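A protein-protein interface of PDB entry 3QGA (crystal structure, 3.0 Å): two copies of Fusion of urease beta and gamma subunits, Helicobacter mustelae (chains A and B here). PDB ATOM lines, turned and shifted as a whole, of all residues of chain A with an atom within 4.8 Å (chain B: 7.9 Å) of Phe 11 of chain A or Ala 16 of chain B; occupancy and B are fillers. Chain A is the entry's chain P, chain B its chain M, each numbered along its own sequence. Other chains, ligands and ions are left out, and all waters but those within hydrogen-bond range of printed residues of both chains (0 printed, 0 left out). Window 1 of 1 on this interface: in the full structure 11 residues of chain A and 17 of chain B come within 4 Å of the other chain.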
ATOM      1  N   FME A   1     -11.230  -1.830 -27.215  1.00  0.00           N
ATOM      2  CN  FME A   1     -10.491  -2.106 -28.293  1.00  0.00           C
ATOM      3  O1  FME A   1     -10.956  -2.585 -29.341  1.00  0.00           O
ATOM      4  CA  FME A   1     -10.662  -1.274 -25.981  1.00  0.00           C
ATOM      5  CB  FME A   1     -11.759  -1.048 -24.924  1.00  0.00           C
ATOM      6  CG  FME A   1     -12.619   0.166 -25.162  1.00  0.00           C
ATOM      7  SD  FME A   1     -13.717   0.474 -23.751  1.00  0.00           S
ATOM      8  CE  FME A   1     -12.699   1.483 -22.782  1.00  0.00           C
ATOM      9  C   FME A   1      -9.593  -2.178 -25.376  1.00  0.00           C
ATOM     10  O   FME A   1      -8.586  -1.668 -24.882  1.00  0.00           O
ATOM     11  N   LEU A   3      -9.858  -4.205 -22.552  1.00  0.00           N
ATOM     12  CA  LEU A   3      -9.763  -3.946 -21.113  1.00  0.00           C
ATOM     13  C   LEU A   3      -9.281  -5.133 -20.274  1.00  0.00           C
ATOM     14  O   LEU A   3      -9.920  -6.191 -20.198  1.00  0.00           O
ATOM     15  CB  LEU A   3     -11.027  -3.297 -20.509  1.00  0.00           C
ATOM     16  CG  LEU A   3     -11.436  -1.913 -21.024  1.00  0.00           C
ATOM     17  CD1 LEU A   3     -12.860  -1.582 -20.594  1.00  0.00           C
ATOM     18  CD2 LEU A   3     -10.461  -0.815 -20.566  1.00  0.00           C
ATOM     19  N   GLU A   7      -7.616  -2.927 -15.360  1.00  0.00           N
ATOM     20  CA  GLU A   7      -8.265  -1.702 -15.849  1.00  0.00           C
ATOM     21  C   GLU A   7      -9.720  -1.650 -15.342  1.00  0.00           C
ATOM     22  O   GLU A   7     -10.181  -0.585 -14.928  1.00  0.00           O
ATOM     23  CB  GLU A   7      -8.190  -1.581 -17.383  1.00  0.00           C
ATOM     24  CG  GLU A   7      -6.972  -0.824 -17.897  1.00  0.00           C
ATOM     25  CD  GLU A   7      -6.826  -0.745 -19.408  1.00  0.00           C
ATOM     26  OE1 GLU A   7      -7.240   0.282 -19.993  1.00  0.00           O
ATOM     27  OE2 GLU A   7      -6.271  -1.696 -20.006  1.00  0.00           O
ATOM     28  N   GLN A   8     -10.407  -2.819 -15.303  1.00  0.00           N
ATOM     29  CA  GLN A   8     -11.785  -2.966 -14.805  1.00  0.00           C
ATOM     30  C   GLN A   8     -11.884  -2.572 -13.321  1.00  0.00           C
ATOM     31  O   GLN A   8     -12.872  -1.948 -12.921  1.00  0.00           O
ATOM     32  CB  GLN A   8     -12.307  -4.401 -15.040  1.00  0.00           C
ATOM     33  CG  GLN A   8     -12.523  -4.746 -16.520  1.00  0.00           C
ATOM     34  CD  GLN A   8     -12.711  -6.223 -16.792  1.00  0.00           C
ATOM     35  OE1 GLN A   8     -11.885  -6.870 -17.460  1.00  0.00           O
ATOM     36  NE2 GLN A   8     -13.829  -6.783 -16.335  1.00  0.00           N
ATOM     37  N   GLU A   9     -10.838  -2.909 -12.523  1.00  0.00           N
ATOM     38  CA  GLU A   9     -10.717  -2.586 -11.091  1.00  0.00           C
ATOM     39  C   GLU A   9     -10.619  -1.081 -10.923  1.00  0.00           C
ATOM     40  O   GLU A   9     -11.352  -0.503 -10.119  1.00  0.00           O
ATOM     41  CB  GLU A   9      -9.447  -3.205 -10.485  1.00  0.00           C
ATOM     42  CG  GLU A   9      -9.489  -4.702 -10.221  1.00  0.00           C
ATOM     43  CD  GLU A   9      -8.257  -5.238  -9.515  1.00  0.00           C
ATOM     44  OE1 GLU A   9      -7.828  -4.616  -8.514  1.00  0.00           O
ATOM     45  OE2 GLU A   9      -7.735  -6.295  -9.939  1.00  0.00           O
ATOM     46  N   LYS A  10      -9.717  -0.440 -11.704  1.00  0.00           N
ATOM     47  CA  LYS A  10      -9.458   1.005 -11.664  1.00  0.00           C
ATOM     48  C   LYS A  10     -10.695   1.853 -11.959  1.00  0.00           C
ATOM     49  O   LYS A  10     -10.843   2.914 -11.356  1.00  0.00           O
ATOM     50  CB  LYS A  10      -8.242   1.400 -12.538  1.00  0.00           C
ATOM     51  CG  LYS A  10      -6.906   0.735 -12.149  1.00  0.00           C
ATOM     52  CD  LYS A  10      -6.206   1.351 -10.940  1.00  0.00           C
ATOM     53  CE  LYS A  10      -5.034   0.494 -10.511  1.00  0.00           C
ATOM     54  NZ  LYS A  10      -4.446   0.939  -9.213  1.00  0.00           N
ATOM     55  N   PHE A  11     -11.612   1.365 -12.829  1.00  0.00           N
ATOM     56  CA  PHE A  11     -12.872   2.064 -13.126  1.00  0.00           C
ATOM     57  C   PHE A  11     -13.738   2.187 -11.867  1.00  0.00           C
ATOM     58  O   PHE A  11     -14.260   3.269 -11.577  1.00  0.00           O
ATOM     59  CB  PHE A  11     -13.642   1.375 -14.257  1.00  0.00           C
ATOM     60  CG  PHE A  11     -13.194   1.815 -15.623  1.00  0.00           C
ATOM     61  CD1 PHE A  11     -13.440   3.105 -16.070  1.00  0.00           C
ATOM     62  CD2 PHE A  11     -12.526   0.937 -16.469  1.00  0.00           C
ATOM     63  CE1 PHE A  11     -12.998   3.513 -17.326  1.00  0.00           C
ATOM     64  CE2 PHE A  11     -12.100   1.345 -17.729  1.00  0.00           C
ATOM     65  CZ  PHE A  11     -12.333   2.627 -18.147  1.00  0.00           C
ATOM     66  N   LEU A  12     -13.830   1.087 -11.094  1.00  0.00           N
ATOM     67  CA  LEU A  12     -14.573   1.040  -9.834  1.00  0.00           C
ATOM     68  C   LEU A  12     -13.963   2.020  -8.838  1.00  0.00           C
ATOM     69  O   LEU A  12     -14.694   2.830  -8.255  1.00  0.00           O
ATOM     70  CB  LEU A  12     -14.596  -0.393  -9.268  1.00  0.00           C
ATOM     71  CG  LEU A  12     -15.135  -0.598  -7.856  1.00  0.00           C
ATOM     72  CD1 LEU A  12     -16.635  -0.284  -7.768  1.00  0.00           C
ATOM     73  CD2 LEU A  12     -14.815  -2.013  -7.369  1.00  0.00           C
ATOM     74  N   LEU A  13     -12.619   1.969  -8.678  1.00  0.00           N
ATOM     75  CA  LEU A  13     -11.890   2.875  -7.800  1.00  0.00           C
ATOM     76  C   LEU A  13     -12.150   4.310  -8.204  1.00  0.00           C
ATOM     77  O   LEU A  13     -12.479   5.115  -7.345  1.00  0.00           O
ATOM     78  CB  LEU A  13     -10.380   2.568  -7.801  1.00  0.00           C
ATOM     79  CG  LEU A  13      -9.486   3.508  -6.985  1.00  0.00           C
ATOM     80  CD1 LEU A  13      -9.794   3.433  -5.507  1.00  0.00           C
ATOM     81  CD2 LEU A  13      -8.033   3.209  -7.236  1.00  0.00           C
ATOM     82  N   TYR A  14     -12.045   4.619  -9.508  1.00  0.00           N
ATOM     83  CA  TYR A  14     -12.270   5.962 -10.010  1.00  0.00           C
ATOM     84  C   TYR A  14     -13.708   6.432  -9.803  1.00  0.00           C
ATOM     85  O   TYR A  14     -13.903   7.578  -9.373  1.00  0.00           O
ATOM     86  CB  TYR A  14     -11.796   6.136 -11.462  1.00  0.00           C
ATOM     87  CG  TYR A  14     -11.642   7.595 -11.844  1.00  0.00           C
ATOM     88  CD1 TYR A  14     -10.543   8.340 -11.408  1.00  0.00           C
ATOM     89  CD2 TYR A  14     -12.621   8.249 -12.589  1.00  0.00           C
ATOM     90  CE1 TYR A  14     -10.423   9.697 -11.711  1.00  0.00           C
ATOM     91  CE2 TYR A  14     -12.504   9.603 -12.907  1.00  0.00           C
ATOM     92  CZ  TYR A  14     -11.411  10.325 -12.453  1.00  0.00           C
ATOM     93  OH  TYR A  14     -11.310  11.653 -12.778  1.00  0.00           O
ATOM     94  N   TYR A  15     -14.710   5.544 -10.044  1.00  0.00           N
ATOM     95  CA  TYR A  15     -16.103   5.920  -9.806  1.00  0.00           C
ATOM     96  C   TYR A  15     -16.358   6.195  -8.329  1.00  0.00           C
ATOM     97  O   TYR A  15     -17.012   7.190  -8.016  1.00  0.00           O
ATOM     98  CB  TYR A  15     -17.106   4.915 -10.368  1.00  0.00           C
ATOM     99  CG  TYR A  15     -18.541   5.381 -10.185  1.00  0.00           C
ATOM    100  CD1 TYR A  15     -18.994   6.559 -10.770  1.00  0.00           C
ATOM    101  CD2 TYR A  15     -19.436   4.662  -9.395  1.00  0.00           C
ATOM    102  CE1 TYR A  15     -20.301   7.008 -10.578  1.00  0.00           C
ATOM    103  CE2 TYR A  15     -20.745   5.103  -9.193  1.00  0.00           C
ATOM    104  CZ  TYR A  15     -21.171   6.282  -9.780  1.00  0.00           C
ATOM    105  OH  TYR A  15     -22.457   6.727  -9.586  1.00  0.00           O
ATOM    106  N   GLU B   9     -22.164  -4.983 -18.872  1.00  0.00           N
ATOM    107  CA  GLU B   9     -21.030  -4.661 -19.751  1.00  0.00           C
ATOM    108  C   GLU B   9     -21.180  -3.234 -20.244  1.00  0.00           C
ATOM    109  O   GLU B   9     -20.237  -2.449 -20.147  1.00  0.00           O
ATOM    110  CB  GLU B   9     -21.005  -5.580 -20.982  1.00  0.00           C
ATOM    111  CG  GLU B   9     -20.504  -6.994 -20.763  1.00  0.00           C
ATOM    112  CD  GLU B   9     -20.392  -7.814 -22.040  1.00  0.00           C
ATOM    113  OE1 GLU B   9     -19.846  -7.295 -23.043  1.00  0.00           O
ATOM    114  OE2 GLU B   9     -20.828  -8.989 -22.029  1.00  0.00           O
ATOM    115  N   LYS B  10     -22.379  -2.899 -20.771  1.00  0.00           N
ATOM    116  CA  LYS B  10     -22.701  -1.586 -21.327  1.00  0.00           C
ATOM    117  C   LYS B  10     -22.532  -0.430 -20.315  1.00  0.00           C
ATOM    118  O   LYS B  10     -22.116   0.652 -20.718  1.00  0.00           O
ATOM    119  CB  LYS B  10     -24.084  -1.577 -22.012  1.00  0.00           C
ATOM    120  CG  LYS B  10     -24.259  -2.565 -23.171  1.00  0.00           C
ATOM    121  CD  LYS B  10     -23.643  -2.111 -24.489  1.00  0.00           C
ATOM    122  CE  LYS B  10     -23.678  -3.234 -25.507  1.00  0.00           C
ATOM    123  NZ  LYS B  10     -22.885  -2.930 -26.740  1.00  0.00           N
ATOM    124  N   PHE B  11     -22.780  -0.673 -19.005  1.00  0.00           N
ATOM    125  CA  PHE B  11     -22.573   0.335 -17.964  1.00  0.00           C
ATOM    126  C   PHE B  11     -21.096   0.722 -17.874  1.00  0.00           C
ATOM    127  O   PHE B  11     -20.775   1.912 -17.813  1.00  0.00           O
ATOM    128  CB  PHE B  11     -23.086  -0.147 -16.610  1.00  0.00           C
ATOM    129  CG  PHE B  11     -24.555   0.109 -16.413  1.00  0.00           C
ATOM    130  CD1 PHE B  11     -25.035   1.400 -16.256  1.00  0.00           C
ATOM    131  CD2 PHE B  11     -25.460  -0.942 -16.372  1.00  0.00           C
ATOM    132  CE1 PHE B  11     -26.404   1.639 -16.121  1.00  0.00           C
ATOM    133  CE2 PHE B  11     -26.826  -0.706 -16.197  1.00  0.00           C
ATOM    134  CZ  PHE B  11     -27.291   0.581 -16.092  1.00  0.00           C
ATOM    135  N   LEU B  12     -20.197  -0.284 -17.935  1.00  0.00           N
ATOM    136  CA  LEU B  12     -18.749  -0.081 -17.919  1.00  0.00           C
ATOM    137  C   LEU B  12     -18.335   0.731 -19.137  1.00  0.00           C
ATOM    138  O   LEU B  12     -17.629   1.736 -18.983  1.00  0.00           O
ATOM    139  CB  LEU B  12     -18.005  -1.433 -17.883  1.00  0.00           C
ATOM    140  CG  LEU B  12     -16.484  -1.402 -18.065  1.00  0.00           C
ATOM    141  CD1 LEU B  12     -15.791  -0.708 -16.861  1.00  0.00           C
ATOM    142  CD2 LEU B  12     -15.940  -2.814 -18.374  1.00  0.00           C
ATOM    143  N   LEU B  13     -18.809   0.317 -20.336  1.00  0.00           N
ATOM    144  CA  LEU B  13     -18.526   1.022 -21.586  1.00  0.00           C
ATOM    145  C   LEU B  13     -18.989   2.468 -21.491  1.00  0.00           C
ATOM    146  O   LEU B  13     -18.227   3.366 -21.828  1.00  0.00           O
ATOM    147  CB  LEU B  13     -19.176   0.317 -22.794  1.00  0.00           C
ATOM    148  CG  LEU B  13     -19.029   1.004 -24.154  1.00  0.00           C
ATOM    149  CD1 LEU B  13     -17.575   1.057 -24.599  1.00  0.00           C
ATOM    150  CD2 LEU B  13     -19.877   0.318 -25.190  1.00  0.00           C
ATOM    151  N   TYR B  14     -20.215   2.688 -20.992  1.00  0.00           N
ATOM    152  CA  TYR B  14     -20.764   4.025 -20.853  1.00  0.00           C
ATOM    153  C   TYR B  14     -19.992   4.868 -19.848  1.00  0.00           C
ATOM    154  O   TYR B  14     -19.717   6.037 -20.143  1.00  0.00           O
ATOM    155  CB  TYR B  14     -22.281   4.021 -20.590  1.00  0.00           C
ATOM    156  CG  TYR B  14     -22.913   5.372 -20.855  1.00  0.00           C
ATOM    157  CD1 TYR B  14     -23.176   5.798 -22.155  1.00  0.00           C
ATOM    158  CD2 TYR B  14     -23.192   6.250 -19.812  1.00  0.00           C
ATOM    159  CE1 TYR B  14     -23.723   7.056 -22.408  1.00  0.00           C
ATOM    160  CE2 TYR B  14     -23.736   7.510 -20.052  1.00  0.00           C
ATOM    161  CZ  TYR B  14     -23.995   7.912 -21.352  1.00  0.00           C
ATOM    162  OH  TYR B  14     -24.533   9.156 -21.577  1.00  0.00           O
ATOM    163  N   TYR B  15     -19.580   4.270 -18.703  1.00  0.00           N
ATOM    164  CA  TYR B  15     -18.790   5.011 -17.721  1.00  0.00           C
ATOM    165  C   TYR B  15     -17.440   5.415 -18.282  1.00  0.00           C
ATOM    166  O   TYR B  15     -17.036   6.571 -18.104  1.00  0.00           O
ATOM    167  CB  TYR B  15     -18.659   4.297 -16.374  1.00  0.00           C
ATOM    168  CG  TYR B  15     -17.916   5.142 -15.355  1.00  0.00           C
ATOM    169  CD1 TYR B  15     -18.397   6.393 -14.971  1.00  0.00           C
ATOM    170  CD2 TYR B  15     -16.712   4.714 -14.811  1.00  0.00           C
ATOM    171  CE1 TYR B  15     -17.696   7.192 -14.071  1.00  0.00           C
ATOM    172  CE2 TYR B  15     -16.012   5.497 -13.898  1.00  0.00           C
ATOM    173  CZ  TYR B  15     -16.502   6.744 -13.539  1.00  0.00           C
ATOM    174  OH  TYR B  15     -15.820   7.541 -12.648  1.00  0.00           O
ATOM    175  N   ALA B  16     -16.778   4.484 -19.029  1.00  0.00           N
ATOM    176  CA  ALA B  16     -15.501   4.733 -19.726  1.00  0.00           C
ATOM    177  C   ALA B  16     -15.652   5.921 -20.697  1.00  0.00           C
ATOM    178  O   ALA B  16     -14.791   6.798 -20.734  1.00  0.00           O
ATOM    179  CB  ALA B  16     -15.050   3.490 -20.469  1.00  0.00           C
ATOM    180  N   GLY B  17     -16.787   5.980 -21.394  1.00  0.00           N
ATOM    181  CA  GLY B  17     -17.130   7.075 -22.292  1.00  0.00           C
ATOM    182  C   GLY B  17     -17.226   8.392 -21.552  1.00  0.00           C
ATOM    183  O   GLY B  17     -16.688   9.407 -22.016  1.00  0.00           O
ATOM    184  N   GLU B  18     -17.861   8.363 -20.355  1.00  0.00           N
ATOM    185  CA  GLU B  18     -18.016   9.540 -19.500  1.00  0.00           C
ATOM    186  C   GLU B  18     -16.664  10.047 -18.979  1.00  0.00           C
ATOM    187  O   GLU B  18     -16.425  11.252 -19.044  1.00  0.00           O
ATOM    188  CB  GLU B  18     -19.035   9.296 -18.386  1.00  0.00           C
ATOM    189  CG  GLU B  18     -20.448   9.092 -18.910  1.00  0.00           C
ATOM    190  CD  GLU B  18     -21.559   9.740 -18.108  1.00  0.00           C
ATOM    191  OE1 GLU B  18     -22.105  10.761 -18.584  1.00  0.00           O
ATOM    192  OE2 GLU B  18     -21.900   9.219 -17.020  1.00  0.00           O
ATOM    193  N   VAL B  19     -15.752   9.130 -18.562  1.00  0.00           N
ATOM    194  CA  VAL B  19     -14.391   9.480 -18.116  1.00  0.00           C
ATOM    195  C   VAL B  19     -13.609  10.114 -19.288  1.00  0.00           C
ATOM    196  O   VAL B  19     -12.955  11.140 -19.095  1.00  0.00           O
ATOM    197  CB  VAL B  19     -13.634   8.277 -17.505  1.00  0.00           C
ATOM    198  CG1 VAL B  19     -12.214   8.653 -17.100  1.00  0.00           C
ATOM    199  CG2 VAL B  19     -14.385   7.711 -16.311  1.00  0.00           C
ATOM    200  N   ALA B  20     -13.708   9.521 -20.500  1.00  0.00           N
ATOM    201  CA  ALA B  20     -13.064  10.029 -21.707  1.00  0.00           C
ATOM    202  C   ALA B  20     -13.546  11.448 -22.029  1.00  0.00           C
ATOM    203  O   ALA B  20     -12.719  12.312 -22.335  1.00  0.00           O
ATOM    204  CB  ALA B  20     -13.335   9.098 -22.873  1.00  0.00           C
ATOM    205  N   ARG B  21     -14.871  11.695 -21.908  1.00  0.00           N
ATOM    206  CA  ARG B  21     -15.479  13.012 -22.143  1.00  0.00           C
ATOM    207  C   ARG B  21     -14.868  14.059 -21.218  1.00  0.00           C
ATOM    208  O   ARG B  21     -14.526  15.150 -21.678  1.00  0.00           O
ATOM    209  CB  ARG B  21     -17.001  12.964 -21.933  1.00  0.00           C
ATOM    210  CG  ARG B  21     -17.739  12.323 -23.088  1.00  0.00           C
ATOM    211  CD  ARG B  21     -19.117  11.835 -22.710  1.00  0.00           C
ATOM    212  NE  ARG B  21     -19.844  11.374 -23.893  1.00  0.00           N
ATOM    213  CZ  ARG B  21     -21.082  10.901 -23.869  1.00  0.00           C
ATOM    214  NH1 ARG B  21     -21.744  10.812 -22.723  1.00  0.00           N
ATOM    215  NH2 ARG B  21     -21.667  10.505 -24.992  1.00  0.00           N
ATOM    216  N   LYS B  22     -14.705  13.701 -19.921  1.00  0.00           N
ATOM    217  CA  LYS B  22     -14.127  14.535 -18.868  1.00  0.00           C
ATOM    218  C   LYS B  22     -12.691  14.929 -19.239  1.00  0.00           C
ATOM    219  O   LYS B  22     -12.349  16.113 -19.192  1.00  0.00           O
ATOM    220  CB  LYS B  22     -14.187  13.789 -17.516  1.00  0.00           C
ATOM    221  CG  LYS B  22     -13.714  14.595 -16.316  1.00  0.00           C
ATOM    222  CD  LYS B  22     -13.657  13.761 -15.045  1.00  0.00           C
ATOM    223  CE  LYS B  22     -12.719  14.410 -14.062  1.00  0.00           C
ATOM    224  NZ  LYS B  22     -12.898  13.854 -12.701  1.00  0.00           N
ATOM    225  N   ARG B  23     -11.880  13.946 -19.657  1.00  0.00           N
ATOM    226  CA  ARG B  23     -10.481  14.133 -20.045  1.00  0.00           C
ATOM    227  C   ARG B  23     -10.328  15.033 -21.280  1.00  0.00           C
ATOM    228  O   ARG B  23      -9.401  15.846 -21.322  1.00  0.00           O
ATOM    229  CB  ARG B  23      -9.781  12.775 -20.212  1.00  0.00           C
ATOM    230  CG  ARG B  23      -9.702  12.037 -18.896  1.00  0.00           C
ATOM    231  CD  ARG B  23      -9.055  10.687 -18.963  1.00  0.00           C
ATOM    232  NE  ARG B  23      -8.659  10.257 -17.623  1.00  0.00           N
ATOM    233  CZ  ARG B  23      -8.161   9.063 -17.326  1.00  0.00           C
ATOM    234  NH1 ARG B  23      -7.964   8.160 -18.281  1.00  0.00           N
ATOM    235  NH2 ARG B  23      -7.823   8.772 -16.076  1.00  0.00           N
ATOM    236  N   LEU B  30      -6.978  12.194 -26.342  1.00  0.00           N
ATOM    237  CA  LEU B  30      -7.444  10.858 -25.982  1.00  0.00           C
ATOM    238  C   LEU B  30      -6.582   9.735 -26.572  1.00  0.00           C
ATOM    239  O   LEU B  30      -6.056   9.872 -27.681  1.00  0.00           O
ATOM    240  CB  LEU B  30      -8.923  10.665 -26.371  1.00  0.00           C
ATOM    241  CG  LEU B  30      -9.948  11.656 -25.805  1.00  0.00           C
ATOM    242  CD1 LEU B  30     -11.323  11.337 -26.310  1.00  0.00           C
ATOM    243  CD2 LEU B  30      -9.953  11.667 -24.283  1.00  0.00           C
ATOM    244  N   PRO B  33      -8.129   3.350 -26.030  1.00  0.00           N
ATOM    245  CA  PRO B  33      -9.384   2.982 -25.359  1.00  0.00           C
ATOM    246  C   PRO B  33     -10.318   4.148 -25.032  1.00  0.00           C
ATOM    247  O   PRO B  33     -11.538   3.975 -25.106  1.00  0.00           O
ATOM    248  CB  PRO B  33      -8.911   2.219 -24.120  1.00  0.00           C
ATOM    249  CG  PRO B  33      -7.565   2.721 -23.859  1.00  0.00           C
ATOM    250  CD  PRO B  33      -6.966   2.975 -25.198  1.00  0.00           C
ATOM    251  N   GLU B  34      -9.759   5.328 -24.703  1.00  0.00           N
ATOM    252  CA  GLU B  34     -10.541   6.527 -24.399  1.00  0.00           C
ATOM    253  C   GLU B  34     -11.339   6.959 -25.633  1.00  0.00           C
ATOM    254  O   GLU B  34     -12.548   7.188 -25.516  1.00  0.00           O
ATOM    255  CB  GLU B  34      -9.642   7.669 -23.923  1.00  0.00           C
ATOM    256  CG  GLU B  34      -9.093   7.496 -22.514  1.00  0.00           C
ATOM    257  CD  GLU B  34      -7.991   8.465 -22.121  1.00  0.00           C
ATOM    258  OE1 GLU B  34      -7.550   9.260 -22.986  1.00  0.00           O
ATOM    259  OE2 GLU B  34      -7.571   8.433 -20.941  1.00  0.00           O
ATOM    260  N   ALA B  35     -10.681   6.997 -26.822  1.00  0.00           N
ATOM    261  CA  ALA B  35     -11.299   7.375 -28.097  1.00  0.00           C
ATOM    262  C   ALA B  35     -12.464   6.460 -28.472  1.00  0.00           C
ATOM    263  O   ALA B  35     -13.532   6.945 -28.861  1.00  0.00           O
ATOM    264  CB  ALA B  35     -10.260   7.406 -29.201  1.00  0.00           C
ATOM    265  N   ILE B  36     -12.276   5.138 -28.315  1.00  0.00           N
ATOM    266  CA  ILE B  36     -13.302   4.128 -28.588  1.00  0.00           C
ATOM    267  C   ILE B  36     -14.516   4.325 -27.651  1.00  0.00           C
ATOM    268  O   ILE B  36     -15.648   4.344 -28.129  1.00  0.00           O
ATOM    269  CB  ILE B  36     -12.691   2.704 -28.499  1.00  0.00           C
ATOM    270  CG1 ILE B  36     -11.747   2.441 -29.683  1.00  0.00           C
ATOM    271  CG2 ILE B  36     -13.774   1.647 -28.426  1.00  0.00           C
ATOM    272  CD1 ILE B  36     -10.713   1.455 -29.410  1.00  0.00           C
ATOM    273  N   ALA B  37     -14.273   4.511 -26.342  1.00  0.00           N
ATOM    274  CA  ALA B  37     -15.329   4.716 -25.357  1.00  0.00           C
ATOM    275  C   ALA B  37     -16.077   6.026 -25.575  1.00  0.00           C
ATOM    276  O   ALA B  37     -17.298   6.058 -25.410  1.00  0.00           O
ATOM    277  CB  ALA B  37     -14.756   4.667 -23.959  1.00  0.00           C
ATOM    278  N   TYR B  38     -15.356   7.098 -25.974  1.00  0.00           N
ATOM    279  CA  TYR B  38     -15.951   8.413 -26.243  1.00  0.00           C
ATOM    280  C   TYR B  38     -16.971   8.325 -27.383  1.00  0.00           C
ATOM    281  O   TYR B  38     -18.088   8.846 -27.256  1.00  0.00           O
ATOM    282  CB  TYR B  38     -14.856   9.448 -26.539  1.00  0.00           C
ATOM    283  CG  TYR B  38     -15.361  10.823 -26.917  1.00  0.00           C
ATOM    284  CD1 TYR B  38     -15.595  11.790 -25.947  1.00  0.00           C
ATOM    285  CD2 TYR B  38     -15.528  11.185 -28.251  1.00  0.00           C
ATOM    286  CE1 TYR B  38     -16.019  13.076 -26.291  1.00  0.00           C
ATOM    287  CE2 TYR B  38     -15.957  12.467 -28.607  1.00  0.00           C
ATOM    288  CZ  TYR B  38     -16.195  13.415 -27.623  1.00  0.00           C
ATOM    289  OH  TYR B  38     -16.597  14.693 -27.959  1.00  0.00           O
ATOM    290  N   SER B  40     -18.347   5.430 -28.565  1.00  0.00           N
ATOM    291  CA  SER B  40     -19.337   4.444 -28.152  1.00  0.00           C
ATOM    292  C   SER B  40     -20.463   5.063 -27.325  1.00  0.00           C
ATOM    293  O   SER B  40     -21.634   4.822 -27.615  1.00  0.00           O
ATOM    294  CB  SER B  40     -18.670   3.302 -27.402  1.00  0.00           C
ATOM    295  OG  SER B  40     -17.770   2.629 -28.263  1.00  0.00           O
ATOM    296  N   ALA B  41     -20.106   5.900 -26.336  1.00  0.00           N
ATOM    297  CA  ALA B  41     -21.067   6.593 -25.482  1.00  0.00           C
ATOM    298  C   ALA B  41     -21.960   7.533 -26.316  1.00  0.00           C
ATOM    299  O   ALA B  41     -23.169   7.578 -26.070  1.00  0.00           O
ATOM    300  CB  ALA B  41     -20.342   7.354 -24.391  1.00  0.00           C
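The side-chain hydroxyl (OH) of Tyr 15 of chain B sits close to the backbone NH (N) of Tyr 15 of chain A, at 3.5 Å.
The side-chain hydroxyl (OH) of Tyr 14 of chain A is in hydrogen-bond range of the side-chain amino group (NZ) of Lys 22 of chain B (2.7 Å).
O of Ile 36 of chain B lies within hydrogen-bond range of OG of Ser 40 of chain B, at 2.7 Å.
The side-chain amide oxygen (OE1) of Gln 8 of chain A sits close to the backbone carbonyl oxygen (O) of Leu 3 of chain A (3.4 Å).
Among the printed residues, merely in contact across the chains: Tyr 14 of chain A with Tyr 15 of chain B, FME 1 of chain A with Pro 33 of chain B, Phe 11 of chain A with Tyr 15 of chain B, Phe 11 of chain A with Ala 16 of chain B, Phe 11 of chain A with Leu 12 of chain B, FME 1 of chain A with Ile 36 of chain B, FME 1 of chain A with Ala 16 of chain B, FME 1 of chain A with Ala 37 of chain B, Leu 3 of chain A with Leu 12 of chain B and FME 1 of chain A with Leu 13 of chain B.
Phe 11 of chain A touches Leu 12 of chain B, but with the chains exchanged Leu 12 of chain A does not touch Phe 11 of chain B (9.7 Å).
Phe 11 of chain A touches Tyr 15 of chain B, but with the chains exchanged Tyr 15 of chain A does not touch Phe 11 of chain B (8.6 Å).
Tyr 14 of chain A touches Tyr 15 of chain B, but with the chains exchanged Tyr 15 of chain A does not touch Tyr 14 of chain B (9.3 Å).
Tyr 15 of chain A touches its own counterpart, Tyr 15 of chain B.
7 positions are printed for both chains.
Of the 12 pairs that touch across the chains among the printed residues, 1 has its exchanged pair printed and touching as well.
Of the 24 printed residues of chain B, 8 touch a printed residue of chain A.
Hydrophobic or aromatic side chains of chain B within 4 Å of the printed part of chain A: Leu 12, Leu 13, Tyr 15, Ala 16, Pro 33, Ile 36 and Ala 37.
Of the 11 printed residues of chain A, 5 touch a printed residue of chain B.
Printed residues of chain A that touch a printed residue of chain B: FME 1, Leu 3, Phe 11, Tyr 14 and Tyr 15.
Hydrophobic or aromatic side chains of chain A that line the printed part of chain B: Leu 3, Phe 11, Tyr 14 and Tyr 15.
Along chain A the printed residues that touch a printed residue of chain B span positions 1 to 15.
Among the printed residues, 12 pairs touch across the chains.
Among the printed residues, no Asp or Glu carboxylate lies within 4 Å of a Lys or Arg side-chain nitrogen of the other chain.
Gln 8 of chain A touches none of the printed residues of chain B.
Of chain B, only Leu 12, Tyr 15 and Ala 16 come within 4 Å of Phe 11 of chain A.
Of the printed residues of chain A, Leu 12 of chain B touches Leu 3 and Phe 11.
Of the printed residues of chain A, Lys 22 of chain B touches Tyr 14.
Of the printed residues of chain A, Pro 33 of chain B touches FME 1 (3.6 Å).
The nearest printed residue of chain A that does not touch Ala 16 of chain B is Leu 3 of chain A (5.5 Å).
The nearest printed residue of chain B that does not touch Tyr 15 of chain A is Val 19 of chain B (6.6 Å).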
